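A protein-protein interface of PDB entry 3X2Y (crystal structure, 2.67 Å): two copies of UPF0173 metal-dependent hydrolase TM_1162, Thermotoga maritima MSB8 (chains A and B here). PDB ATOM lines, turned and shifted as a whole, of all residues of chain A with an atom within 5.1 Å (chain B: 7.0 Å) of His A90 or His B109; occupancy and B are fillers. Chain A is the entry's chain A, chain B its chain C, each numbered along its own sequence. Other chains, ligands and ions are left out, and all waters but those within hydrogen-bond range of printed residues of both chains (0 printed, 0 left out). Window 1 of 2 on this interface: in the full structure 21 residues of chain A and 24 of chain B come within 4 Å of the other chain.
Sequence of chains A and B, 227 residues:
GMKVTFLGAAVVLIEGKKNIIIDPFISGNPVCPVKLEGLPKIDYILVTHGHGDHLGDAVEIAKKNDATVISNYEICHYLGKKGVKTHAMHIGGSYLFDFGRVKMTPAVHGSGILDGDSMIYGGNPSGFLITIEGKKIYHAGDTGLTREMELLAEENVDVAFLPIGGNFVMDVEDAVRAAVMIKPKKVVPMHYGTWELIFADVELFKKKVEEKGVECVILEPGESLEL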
ATOM      1  N   ASN A  72      16.595 -36.790 -16.476  1.00  0.00           N
ATOM      2  CA  ASN A  72      16.140 -35.707 -17.344  1.00  0.00           C
ATOM      3  C   ASN A  72      15.970 -36.188 -18.797  1.00  0.00           C
ATOM      4  O   ASN A  72      16.406 -37.283 -19.153  1.00  0.00           O
ATOM      5  CB  ASN A  72      17.035 -34.455 -17.218  1.00  0.00           C
ATOM      6  CG  ASN A  72      18.417 -34.626 -17.841  1.00  0.00           C
ATOM      7  OD1 ASN A  72      18.561 -35.151 -18.945  1.00  0.00           O
ATOM      8  ND2 ASN A  72      19.441 -34.134 -17.147  1.00  0.00           N
ATOM      9  N   TYR A  73      15.316 -35.370 -19.615  1.00  0.00           N
ATOM     10  CA  TYR A  73      14.976 -35.746 -20.991  1.00  0.00           C
ATOM     11  C   TYR A  73      16.192 -36.148 -21.836  1.00  0.00           C
ATOM     12  O   TYR A  73      16.129 -37.120 -22.589  1.00  0.00           O
ATOM     13  CB  TYR A  73      14.192 -34.611 -21.672  1.00  0.00           C
ATOM     14  CG  TYR A  73      14.136 -34.707 -23.182  1.00  0.00           C
ATOM     15  CD1 TYR A  73      13.353 -35.671 -23.812  1.00  0.00           C
ATOM     16  CD2 TYR A  73      14.872 -33.833 -23.980  1.00  0.00           C
ATOM     17  CE1 TYR A  73      13.305 -35.764 -25.195  1.00  0.00           C
ATOM     18  CE2 TYR A  73      14.832 -33.917 -25.363  1.00  0.00           C
ATOM     19  CZ  TYR A  73      14.047 -34.883 -25.965  1.00  0.00           C
ATOM     20  OH  TYR A  73      14.008 -34.963 -27.338  1.00  0.00           O
ATOM     21  N   GLU A  74      17.295 -35.414 -21.699  1.00  0.00           N
ATOM     22  CA  GLU A  74      18.481 -35.647 -22.532  1.00  0.00           C
ATOM     23  C   GLU A  74      19.194 -36.937 -22.140  1.00  0.00           C
ATOM     24  O   GLU A  74      19.678 -37.671 -23.007  1.00  0.00           O
ATOM     25  CB  GLU A  74      19.462 -34.469 -22.453  1.00  0.00           C
ATOM     26  CG  GLU A  74      18.973 -33.197 -23.141  1.00  0.00           C
ATOM     27  CD  GLU A  74      18.014 -32.369 -22.297  1.00  0.00           C
ATOM     28  OE1 GLU A  74      17.682 -32.788 -21.171  1.00  0.00           O
ATOM     29  OE2 GLU A  74      17.586 -31.292 -22.757  1.00  0.00           O
ATOM     30  N   ALA A  88      11.313 -40.035 -18.567  1.00  0.00           N
ATOM     31  CA  ALA A  88      11.911 -38.712 -18.642  1.00  0.00           C
ATOM     32  C   ALA A  88      11.186 -37.708 -17.746  1.00  0.00           C
ATOM     33  O   ALA A  88       9.974 -37.781 -17.586  1.00  0.00           O
ATOM     34  CB  ALA A  88      11.911 -38.226 -20.080  1.00  0.00           C
ATOM     35  N   MET A  89      11.953 -36.795 -17.152  1.00  0.00           N
ATOM     36  CA  MET A  89      11.421 -35.681 -16.369  1.00  0.00           C
ATOM     37  C   MET A  89      12.280 -34.461 -16.655  1.00  0.00           C
ATOM     38  O   MET A  89      13.114 -34.494 -17.560  1.00  0.00           O
ATOM     39  CB  MET A  89      11.476 -35.994 -14.875  1.00  0.00           C
ATOM     40  CG  MET A  89      10.697 -37.217 -14.446  1.00  0.00           C
ATOM     41  SD  MET A  89      10.826 -37.524 -12.669  1.00  0.00           S
ATOM     42  CE  MET A  89       9.740 -36.273 -12.019  1.00  0.00           C
ATOM     43  N   HIS A  90      12.069 -33.373 -15.913  1.00  0.00           N
ATOM     44  CA  HIS A  90      13.056 -32.293 -15.879  1.00  0.00           C
ATOM     45  C   HIS A  90      12.995 -31.487 -14.586  1.00  0.00           C
ATOM     46  O   HIS A  90      12.161 -31.760 -13.731  1.00  0.00           O
ATOM     47  CB  HIS A  90      12.958 -31.389 -17.111  1.00  0.00           C
ATOM     48  CG  HIS A  90      14.261 -31.251 -17.835  1.00  0.00           C
ATOM     49  ND1 HIS A  90      14.423 -31.652 -19.142  1.00  0.00           N
ATOM     50  CD2 HIS A  90      15.477 -30.826 -17.417  1.00  0.00           C
ATOM     51  CE1 HIS A  90      15.677 -31.456 -19.507  1.00  0.00           C
ATOM     52  NE2 HIS A  90      16.341 -30.962 -18.476  1.00  0.00           N
ATOM     53  N   ILE A  91      13.879 -30.491 -14.470  1.00  0.00           N
ATOM     54  CA  ILE A  91      14.149 -29.818 -13.209  1.00  0.00           C
ATOM     55  C   ILE A  91      12.864 -29.166 -12.715  1.00  0.00           C
ATOM     56  O   ILE A  91      12.228 -28.403 -13.444  1.00  0.00           O
ATOM     57  CB  ILE A  91      15.230 -28.710 -13.322  1.00  0.00           C
ATOM     58  CG1 ILE A  91      16.483 -29.154 -14.096  1.00  0.00           C
ATOM     59  CG2 ILE A  91      15.625 -28.220 -11.933  1.00  0.00           C
ATOM     60  CD1 ILE A  91      17.086 -30.464 -13.660  1.00  0.00           C
ATOM     61  N   GLY A  92      12.482 -29.485 -11.485  1.00  0.00           N
ATOM     62  CA  GLY A  92      11.274 -28.936 -10.884  1.00  0.00           C
ATOM     63  C   GLY A  92      10.028 -29.755 -11.131  1.00  0.00           C
ATOM     64  O   GLY A  92       9.009 -29.539 -10.476  1.00  0.00           O
ATOM     65  N   GLY A  93      10.097 -30.689 -12.073  1.00  0.00           N
ATOM     66  CA  GLY A  93       8.984 -31.590 -12.347  1.00  0.00           C
ATOM     67  C   GLY A  93       8.925 -32.728 -11.349  1.00  0.00           C
ATOM     68  O   GLY A  93       9.949 -33.171 -10.845  1.00  0.00           O
ATOM     69  N   MET A 104      12.457 -33.826  -9.364  1.00  0.00           N
ATOM     70  CA  MET A 104      13.783 -33.339  -9.735  1.00  0.00           C
ATOM     71  C   MET A 104      14.001 -31.940  -9.172  1.00  0.00           C
ATOM     72  O   MET A 104      13.164 -31.067  -9.361  1.00  0.00           O
ATOM     73  CB  MET A 104      13.942 -33.288 -11.250  1.00  0.00           C
ATOM     74  CG  MET A 104      14.245 -34.626 -11.898  1.00  0.00           C
ATOM     75  SD  MET A 104      14.990 -34.410 -13.528  1.00  0.00           S
ATOM     76  CE  MET A 104      16.194 -35.727 -13.478  1.00  0.00           C
ATOM     77  N   GLY A 123      21.679 -32.695 -20.674  1.00  0.00           N
ATOM     78  CA  GLY A 123      20.773 -31.777 -19.994  1.00  0.00           C
ATOM     79  C   GLY A 123      21.470 -30.956 -18.927  1.00  0.00           C
ATOM     80  O   GLY A 123      22.666 -30.693 -19.016  1.00  0.00           O
ATOM     81  N   ASN A 124      20.712 -30.549 -17.916  1.00  0.00           N
ATOM     82  CA  ASN A 124      21.266 -29.876 -16.749  1.00  0.00           C
ATOM     83  C   ASN A 124      21.288 -30.842 -15.564  1.00  0.00           C
ATOM     84  O   ASN A 124      20.492 -31.787 -15.532  1.00  0.00           O
ATOM     85  CB  ASN A 124      20.455 -28.618 -16.411  1.00  0.00           C
ATOM     86  CG  ASN A 124      20.938 -27.392 -17.165  1.00  0.00           C
ATOM     87  OD1 ASN A 124      22.125 -27.073 -17.161  1.00  0.00           O
ATOM     88  ND2 ASN A 124      20.019 -26.683 -17.797  1.00  0.00           N
ATOM     89  N   HIS B  49      13.971 -22.568 -25.536  1.00  0.00           N
ATOM     90  CA  HIS B  49      14.966 -23.641 -25.452  1.00  0.00           C
ATOM     91  C   HIS B  49      14.843 -24.615 -26.622  1.00  0.00           C
ATOM     92  O   HIS B  49      13.891 -24.553 -27.396  1.00  0.00           O
ATOM     93  CB  HIS B  49      14.858 -24.387 -24.115  1.00  0.00           C
ATOM     94  CG  HIS B  49      13.526 -25.025 -23.878  1.00  0.00           C
ATOM     95  ND1 HIS B  49      12.376 -24.295 -23.677  1.00  0.00           N
ATOM     96  CD2 HIS B  49      13.168 -26.326 -23.779  1.00  0.00           C
ATOM     97  CE1 HIS B  49      11.364 -25.119 -23.476  1.00  0.00           C
ATOM     98  NE2 HIS B  49      11.816 -26.357 -23.530  1.00  0.00           N
ATOM     99  N   HIS B  51      14.236 -27.856 -27.077  1.00  0.00           N
ATOM    100  CA  HIS B  51      13.316 -28.990 -27.163  1.00  0.00           C
ATOM    101  C   HIS B  51      12.304 -28.801 -28.289  1.00  0.00           C
ATOM    102  O   HIS B  51      11.776 -27.702 -28.480  1.00  0.00           O
ATOM    103  CB  HIS B  51      12.589 -29.221 -25.837  1.00  0.00           C
ATOM    104  CG  HIS B  51      13.487 -29.668 -24.725  1.00  0.00           C
ATOM    105  ND1 HIS B  51      13.075 -29.713 -23.412  1.00  0.00           N
ATOM    106  CD2 HIS B  51      14.781 -30.066 -24.725  1.00  0.00           C
ATOM    107  CE1 HIS B  51      14.064 -30.143 -22.654  1.00  0.00           C
ATOM    108  NE2 HIS B  51      15.115 -30.353 -23.425  1.00  0.00           N
ATOM    109  N   ASP B  53       9.206 -29.432 -28.996  1.00  0.00           N
ATOM    110  CA  ASP B  53       7.871 -28.861 -28.788  1.00  0.00           C
ATOM    111  C   ASP B  53       7.902 -27.388 -28.349  1.00  0.00           C
ATOM    112  O   ASP B  53       6.912 -26.866 -27.840  1.00  0.00           O
ATOM    113  CB  ASP B  53       7.055 -29.718 -27.803  1.00  0.00           C
ATOM    114  CG  ASP B  53       7.678 -29.796 -26.432  1.00  0.00           C
ATOM    115  OD1 ASP B  53       8.921 -29.830 -26.341  1.00  0.00           O
ATOM    116  OD2 ASP B  53       6.921 -29.831 -25.441  1.00  0.00           O
ATOM    117  N   HIS B  54       9.044 -26.728 -28.540  1.00  0.00           N
ATOM    118  CA  HIS B  54       9.156 -25.283 -28.353  1.00  0.00           C
ATOM    119  C   HIS B  54       9.869 -24.650 -29.542  1.00  0.00           C
ATOM    120  O   HIS B  54       9.388 -23.679 -30.111  1.00  0.00           O
ATOM    121  CB  HIS B  54       9.880 -24.972 -27.042  1.00  0.00           C
ATOM    122  CG  HIS B  54       9.105 -25.384 -25.835  1.00  0.00           C
ATOM    123  ND1 HIS B  54       8.360 -24.499 -25.088  1.00  0.00           N
ATOM    124  CD2 HIS B  54       8.926 -26.599 -25.269  1.00  0.00           C
ATOM    125  CE1 HIS B  54       7.769 -25.148 -24.102  1.00  0.00           C
ATOM    126  NE2 HIS B  54       8.093 -26.426 -24.193  1.00  0.00           N
ATOM    127  N   ALA B 107      15.907 -19.907 -16.360  1.00  0.00           N
ATOM    128  CA  ALA B 107      14.979 -21.011 -16.182  1.00  0.00           C
ATOM    129  C   ALA B 107      15.767 -22.205 -15.688  1.00  0.00           C
ATOM    130  O   ALA B 107      16.966 -22.299 -15.920  1.00  0.00           O
ATOM    131  CB  ALA B 107      14.287 -21.342 -17.490  1.00  0.00           C
ATOM    132  N   VAL B 108      15.090 -23.114 -15.005  1.00  0.00           N
ATOM    133  CA  VAL B 108      15.709 -24.360 -14.583  1.00  0.00           C
ATOM    134  C   VAL B 108      15.035 -25.477 -15.363  1.00  0.00           C
ATOM    135  O   VAL B 108      13.882 -25.815 -15.121  1.00  0.00           O
ATOM    136  CB  VAL B 108      15.667 -24.566 -13.052  1.00  0.00           C
ATOM    137  CG1 VAL B 108      16.456 -23.463 -12.365  1.00  0.00           C
ATOM    138  CG2 VAL B 108      14.245 -24.608 -12.510  1.00  0.00           C
ATOM    139  N   HIS B 109      15.777 -26.004 -16.334  1.00  0.00           N
ATOM    140  CA  HIS B 109      15.263 -26.927 -17.333  1.00  0.00           C
ATOM    141  C   HIS B 109      16.458 -27.437 -18.157  1.00  0.00           C
ATOM    142  O   HIS B 109      17.595 -27.275 -17.745  1.00  0.00           O
ATOM    143  CB  HIS B 109      14.237 -26.202 -18.218  1.00  0.00           C
ATOM    144  CG  HIS B 109      13.328 -27.122 -18.961  1.00  0.00           C
ATOM    145  ND1 HIS B 109      12.461 -27.982 -18.324  1.00  0.00           N
ATOM    146  CD2 HIS B 109      13.166 -27.333 -20.284  1.00  0.00           C
ATOM    147  CE1 HIS B 109      11.800 -28.682 -19.226  1.00  0.00           C
ATOM    148  NE2 HIS B 109      12.209 -28.307 -20.422  1.00  0.00           N
ATOM    149  N   GLY B 110      16.217 -28.068 -19.299  1.00  0.00           N
ATOM    150  CA  GLY B 110      17.291 -28.386 -20.242  1.00  0.00           C
ATOM    151  C   GLY B 110      17.044 -27.689 -21.562  1.00  0.00           C
ATOM    152  O   GLY B 110      16.036 -26.992 -21.718  1.00  0.00           O
ATOM    153  N   SER B 111      17.958 -27.867 -22.511  1.00  0.00           N
ATOM    154  CA  SER B 111      17.814 -27.240 -23.820  1.00  0.00           C
ATOM    155  C   SER B 111      18.508 -28.034 -24.931  1.00  0.00           C
ATOM    156  O   SER B 111      19.286 -27.490 -25.711  1.00  0.00           O
ATOM    157  CB  SER B 111      18.342 -25.807 -23.770  1.00  0.00           C
ATOM    158  OG  SER B 111      18.043 -25.120 -24.968  1.00  0.00           O
ATOM    159  N   GLY B 112      18.205 -29.321 -25.005  1.00  0.00           N
ATOM    160  CA  GLY B 112      18.754 -30.173 -26.051  1.00  0.00           C
ATOM    161  C   GLY B 112      17.995 -30.025 -27.356  1.00  0.00           C
ATOM    162  O   GLY B 112      16.763 -30.023 -27.367  1.00  0.00           O
ATOM    163  N   GLY B 123      22.446 -24.578 -25.630  1.00  0.00           N
ATOM    164  CA  GLY B 123      22.663 -23.620 -24.547  1.00  0.00           C
ATOM    165  C   GLY B 123      21.926 -23.974 -23.262  1.00  0.00           C
ATOM    166  O   GLY B 123      21.688 -25.144 -22.968  1.00  0.00           O
ATOM    167  N   ASN B 124      21.569 -22.951 -22.493  1.00  0.00           N
ATOM    168  CA  ASN B 124      20.706 -23.122 -21.332  1.00  0.00           C
ATOM    169  C   ASN B 124      19.313 -22.575 -21.617  1.00  0.00           C
ATOM    170  O   ASN B 124      19.162 -21.661 -22.422  1.00  0.00           O
ATOM    171  CB  ASN B 124      21.304 -22.439 -20.096  1.00  0.00           C
ATOM    172  CG  ASN B 124      22.320 -23.313 -19.385  1.00  0.00           C
ATOM    173  OD1 ASN B 124      22.091 -24.498 -19.171  1.00  0.00           O
ATOM    174  ND2 ASN B 124      23.440 -22.731 -19.006  1.00  0.00           N
ATOM    175  N   PRO B 125      18.292 -23.137 -20.956  1.00  0.00           N
ATOM    176  CA  PRO B 125      16.915 -22.707 -21.162  1.00  0.00           C
ATOM    177  C   PRO B 125      16.643 -21.321 -20.597  1.00  0.00           C
ATOM    178  O   PRO B 125      17.344 -20.870 -19.701  1.00  0.00           O
ATOM    179  CB  PRO B 125      16.108 -23.747 -20.384  1.00  0.00           C
ATOM    180  CG  PRO B 125      17.026 -24.164 -19.286  1.00  0.00           C
ATOM    181  CD  PRO B 125      18.386 -24.180 -19.917  1.00  0.00           C
ATOM    182  N   SER B 126      15.609 -20.669 -21.108  1.00  0.00           N
ATOM    183  CA  SER B 126      15.263 -19.325 -20.680  1.00  0.00           C
ATOM    184  C   SER B 126      13.764 -19.104 -20.668  1.00  0.00           C
ATOM    185  O   SER B 126      12.985 -19.988 -21.021  1.00  0.00           O
ATOM    186  CB  SER B 126      15.897 -18.297 -21.620  1.00  0.00           C
ATOM    187  OG  SER B 126      15.125 -18.132 -22.799  1.00  0.00           O
ATOM    188  N   GLY B 141       8.738 -20.009 -20.300  1.00  0.00           N
ATOM    189  CA  GLY B 141       9.267 -21.154 -21.038  1.00  0.00           C
ATOM    190  C   GLY B 141       8.988 -22.409 -20.235  1.00  0.00           C
ATOM    191  O   GLY B 141       8.128 -22.400 -19.346  1.00  0.00           O
ATOM    192  N   ASP B 142       9.709 -23.489 -20.536  1.00  0.00           N
ATOM    193  CA  ASP B 142       9.700 -24.657 -19.662  1.00  0.00           C
ATOM    194  C   ASP B 142      10.637 -24.373 -18.502  1.00  0.00           C
ATOM    195  O   ASP B 142      11.810 -24.061 -18.711  1.00  0.00           O
ATOM    196  CB  ASP B 142      10.176 -25.915 -20.383  1.00  0.00           C
ATOM    197  CG  ASP B 142       9.109 -26.547 -21.246  1.00  0.00           C
ATOM    198  OD1 ASP B 142       7.924 -26.182 -21.120  1.00  0.00           O
ATOM    199  OD2 ASP B 142       9.464 -27.432 -22.051  1.00  0.00           O
ATOM    200  N   THR B 143      10.116 -24.467 -17.285  1.00  0.00           N
ATOM    201  CA  THR B 143      10.929 -24.264 -16.102  1.00  0.00           C
ATOM    202  C   THR B 143      10.274 -24.865 -14.866  1.00  0.00           C
ATOM    203  O   THR B 143       9.056 -25.047 -14.812  1.00  0.00           O
ATOM    204  CB  THR B 143      11.208 -22.770 -15.842  1.00  0.00           C
ATOM    205  OG1 THR B 143      12.141 -22.627 -14.761  1.00  0.00           O
ATOM    206  CG2 THR B 143       9.920 -22.013 -15.510  1.00  0.00           C
ATOM    207  N   GLY B 144      11.114 -25.205 -13.895  1.00  0.00           N
ATOM    208  CA  GLY B 144      10.664 -25.521 -12.563  1.00  0.00           C
ATOM    209  C   GLY B 144      10.624 -24.252 -11.742  1.00  0.00           C
ATOM    210  O   GLY B 144      10.962 -23.172 -12.228  1.00  0.00           O
ATOM    211  N   ASN B 167       5.752 -33.079 -14.151  1.00  0.00           N
ATOM    212  CA  ASN B 167       6.715 -34.032 -14.734  1.00  0.00           C
ATOM    213  C   ASN B 167       7.929 -33.399 -15.439  1.00  0.00           C
ATOM    214  O   ASN B 167       9.065 -33.631 -15.039  1.00  0.00           O
ATOM    215  CB  ASN B 167       6.016 -35.020 -15.674  1.00  0.00           C
ATOM    216  CG  ASN B 167       6.895 -36.206 -16.016  1.00  0.00           C
ATOM    217  OD1 ASN B 167       6.957 -37.188 -15.272  1.00  0.00           O
ATOM    218  ND2 ASN B 167       7.586 -36.118 -17.142  1.00  0.00           N
ATOM    219  N   PHE B 168       7.691 -32.638 -16.505  1.00  0.00           N
ATOM    220  CA  PHE B 168       8.768 -31.916 -17.194  1.00  0.00           C
ATOM    221  C   PHE B 168       8.933 -30.483 -16.672  1.00  0.00           C
ATOM    222  O   PHE B 168       9.977 -29.861 -16.869  1.00  0.00           O
ATOM    223  CB  PHE B 168       8.512 -31.878 -18.703  1.00  0.00           C
ATOM    224  CG  PHE B 168       8.628 -33.214 -19.376  1.00  0.00           C
ATOM    225  CD1 PHE B 168       9.867 -33.806 -19.553  1.00  0.00           C
ATOM    226  CD2 PHE B 168       7.497 -33.873 -19.851  1.00  0.00           C
ATOM    227  CE1 PHE B 168       9.985 -35.035 -20.181  1.00  0.00           C
ATOM    228  CE2 PHE B 168       7.606 -35.105 -20.477  1.00  0.00           C
ATOM    229  CZ  PHE B 168       8.854 -35.686 -20.644  1.00  0.00           C
ATOM    230  N   VAL B 169       7.898 -29.966 -16.016  1.00  0.00           N
ATOM    231  CA  VAL B 169       7.857 -28.575 -15.578  1.00  0.00           C
ATOM    232  C   VAL B 169       7.131 -28.504 -14.238  1.00  0.00           C
ATOM    233  O   VAL B 169       6.786 -29.533 -13.664  1.00  0.00           O
ATOM    234  CB  VAL B 169       7.140 -27.677 -16.621  1.00  0.00           C
ATOM    235  CG1 VAL B 169       7.856 -27.729 -17.965  1.00  0.00           C
ATOM    236  CG2 VAL B 169       5.675 -28.075 -16.784  1.00  0.00           C
ATOM    237  N   MET B 170       6.897 -27.292 -13.745  1.00  0.00           N
ATOM    238  CA  MET B 170       6.137 -27.088 -12.506  1.00  0.00           C
ATOM    239  C   MET B 170       4.774 -27.773 -12.556  1.00  0.00           C
ATOM    240  O   MET B 170       4.204 -27.975 -13.628  1.00  0.00           O
ATOM    241  CB  MET B 170       5.882 -25.598 -12.238  1.00  0.00           C
ATOM    242  CG  MET B 170       7.060 -24.664 -12.434  1.00  0.00           C
ATOM    243  SD  MET B 170       6.568 -22.941 -12.276  1.00  0.00           S
ATOM    244  CE  MET B 170       6.779 -22.817 -10.523  1.00  0.00           C
ATOM    245  N   HIS B 191       1.024 -24.938 -21.192  1.00  0.00           N
ATOM    246  CA  HIS B 191       1.810 -26.176 -21.263  1.00  0.00           C
ATOM    247  C   HIS B 191       1.203 -27.307 -20.420  1.00  0.00           C
ATOM    248  O   HIS B 191       1.922 -28.191 -19.942  1.00  0.00           O
ATOM    249  CB  HIS B 191       3.261 -25.903 -20.838  1.00  0.00           C
ATOM    250  CG  HIS B 191       4.239 -26.943 -21.297  1.00  0.00           C
ATOM    251  ND1 HIS B 191       4.587 -28.030 -20.524  1.00  0.00           N
ATOM    252  CD2 HIS B 191       4.952 -27.054 -22.444  1.00  0.00           C
ATOM    253  CE1 HIS B 191       5.469 -28.768 -21.176  1.00  0.00           C
ATOM    254  NE2 HIS B 191       5.709 -28.197 -22.342  1.00  0.00           N
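Of the 12 printed residues of chain A, 9 touch a printed residue of chain B. Hydrophobic or aromatic side chains of chain A within 4 Å of the printed part of chain B: Tyr A73, Ala A88, Met A89, His A90 and Ile A91. Printed residues of chain B that touch a printed residue of chain A: His B51, Val B108, His B109, Gly B110, Ser B111, Gly B112, Asn B124, Pro B125, Gly B144, Asn B167, Phe B168 and Val B169. Hydrophobic or aromatic side chains of chain B within 4 Å of the printed part of chain A: His B51, Val B108, His B109, Pro B125 and Phe B168.
His A90 touches just these residues of chain B: His B51 (3.8 Å), His B109 (3.5 Å), Gly B110 (3.0 Å), Asn B167 (3.1 Å) and Phe B168 (3.4 Å). His B109 touches just these residues of chain A: His A90 (3.5 Å), Ile A91 (3.9 Å) and Asn A124 (2.5 Å). Of the printed residues of chain A, His B51 touches Tyr A73, Glu A74 and His A90. Printed residues of chain A within 4 Å of Asn B124: Asn A124 (3.3 Å). Of the printed residues of chain A, Gly B112 touches Glu A74. Printed residues of chain B within 4 Å of Tyr A73: His B51 (3.5 Å). The nearest residue of chain B that does not touch His A90 is Val B169 (5.2 Å).
Asn A124 touches its own counterpart, Asn B124. Positions printed for both chains: 123 and 124.
OD1 of Asn A72 sits at hydrogen-bond distance from N of Glu A74 (3.0 Å). O of Met A89 is in hydrogen-bond range of N of Tyr A73. The backbone NH (N) of Met A104 is in hydrogen-bond range of the backbone carbonyl oxygen (O) of Gly A93 (3.0 Å). N of His B51 sits close to O of Gly B112 (3.3 Å). The backbone NH (N) of Val B108 lies within hydrogen-bond range of the side-chain hydroxyl (OG1) of Thr B143, at 3.0 Å. A ring nitrogen (ND1) of His B109 lies close to the backbone carbonyl oxygen (O) of Phe B168 (3.4 Å).
A ring nitrogen (NE2) of His B51 sits at hydrogen-bond distance from the side-chain carboxylate of Glu A74. The backbone NH of Ser B111 lies within hydrogen-bond range of the side-chain carboxylate of Glu A74, at 3.5 Å. OE2 of Glu A74 is in hydrogen-bond range of N of Gly B112 (3.1 Å). O of Ala A88 sits at hydrogen-bond distance from ND2 of Asn B167 (2.9 Å). NE2 of His A90 sits at hydrogen-bond distance from N of Gly B110 (3.0 Å). O of Asn B167 sits at hydrogen-bond distance from N of His A90 (3.1 Å). The backbone carbonyl oxygen of Ile A91 lies close to the backbone NH of Gly B144 (3.4 Å). ND2 of Asn A124 sits at hydrogen-bond distance from O of His B109 (2.5 Å). The side-chain amide oxygen (OD1) of Asn B124 sits close to the side-chain amide oxygen (OD1) of Asn A124, 3.3 Å away. The backbone carbonyl oxygen (O) of Val B108 lies close to the backbone carbonyl oxygen (O) of Ile A91, at 3.5 Å.
His B51 touches Tyr A73 (NE2 to CD2, 3.5 Å). Gly B110 touches Glu A74 (C to OE2, 3.8 Å). CE1 of Phe B168 touches CB of Ala A88, 3.7 Å away. Asn B167 touches Met A89. Met A89 touches Phe B168 (C to CD1, 3.8 Å). CE1 of His B51 touches CE1 of His A90 (3.8 Å). Val B169 touches Gly A92. Gly A93 touches Asn B167 (CA to O, 3.4 Å). Gly A93 touches Val B169. Asn A124 touches Pro B125.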
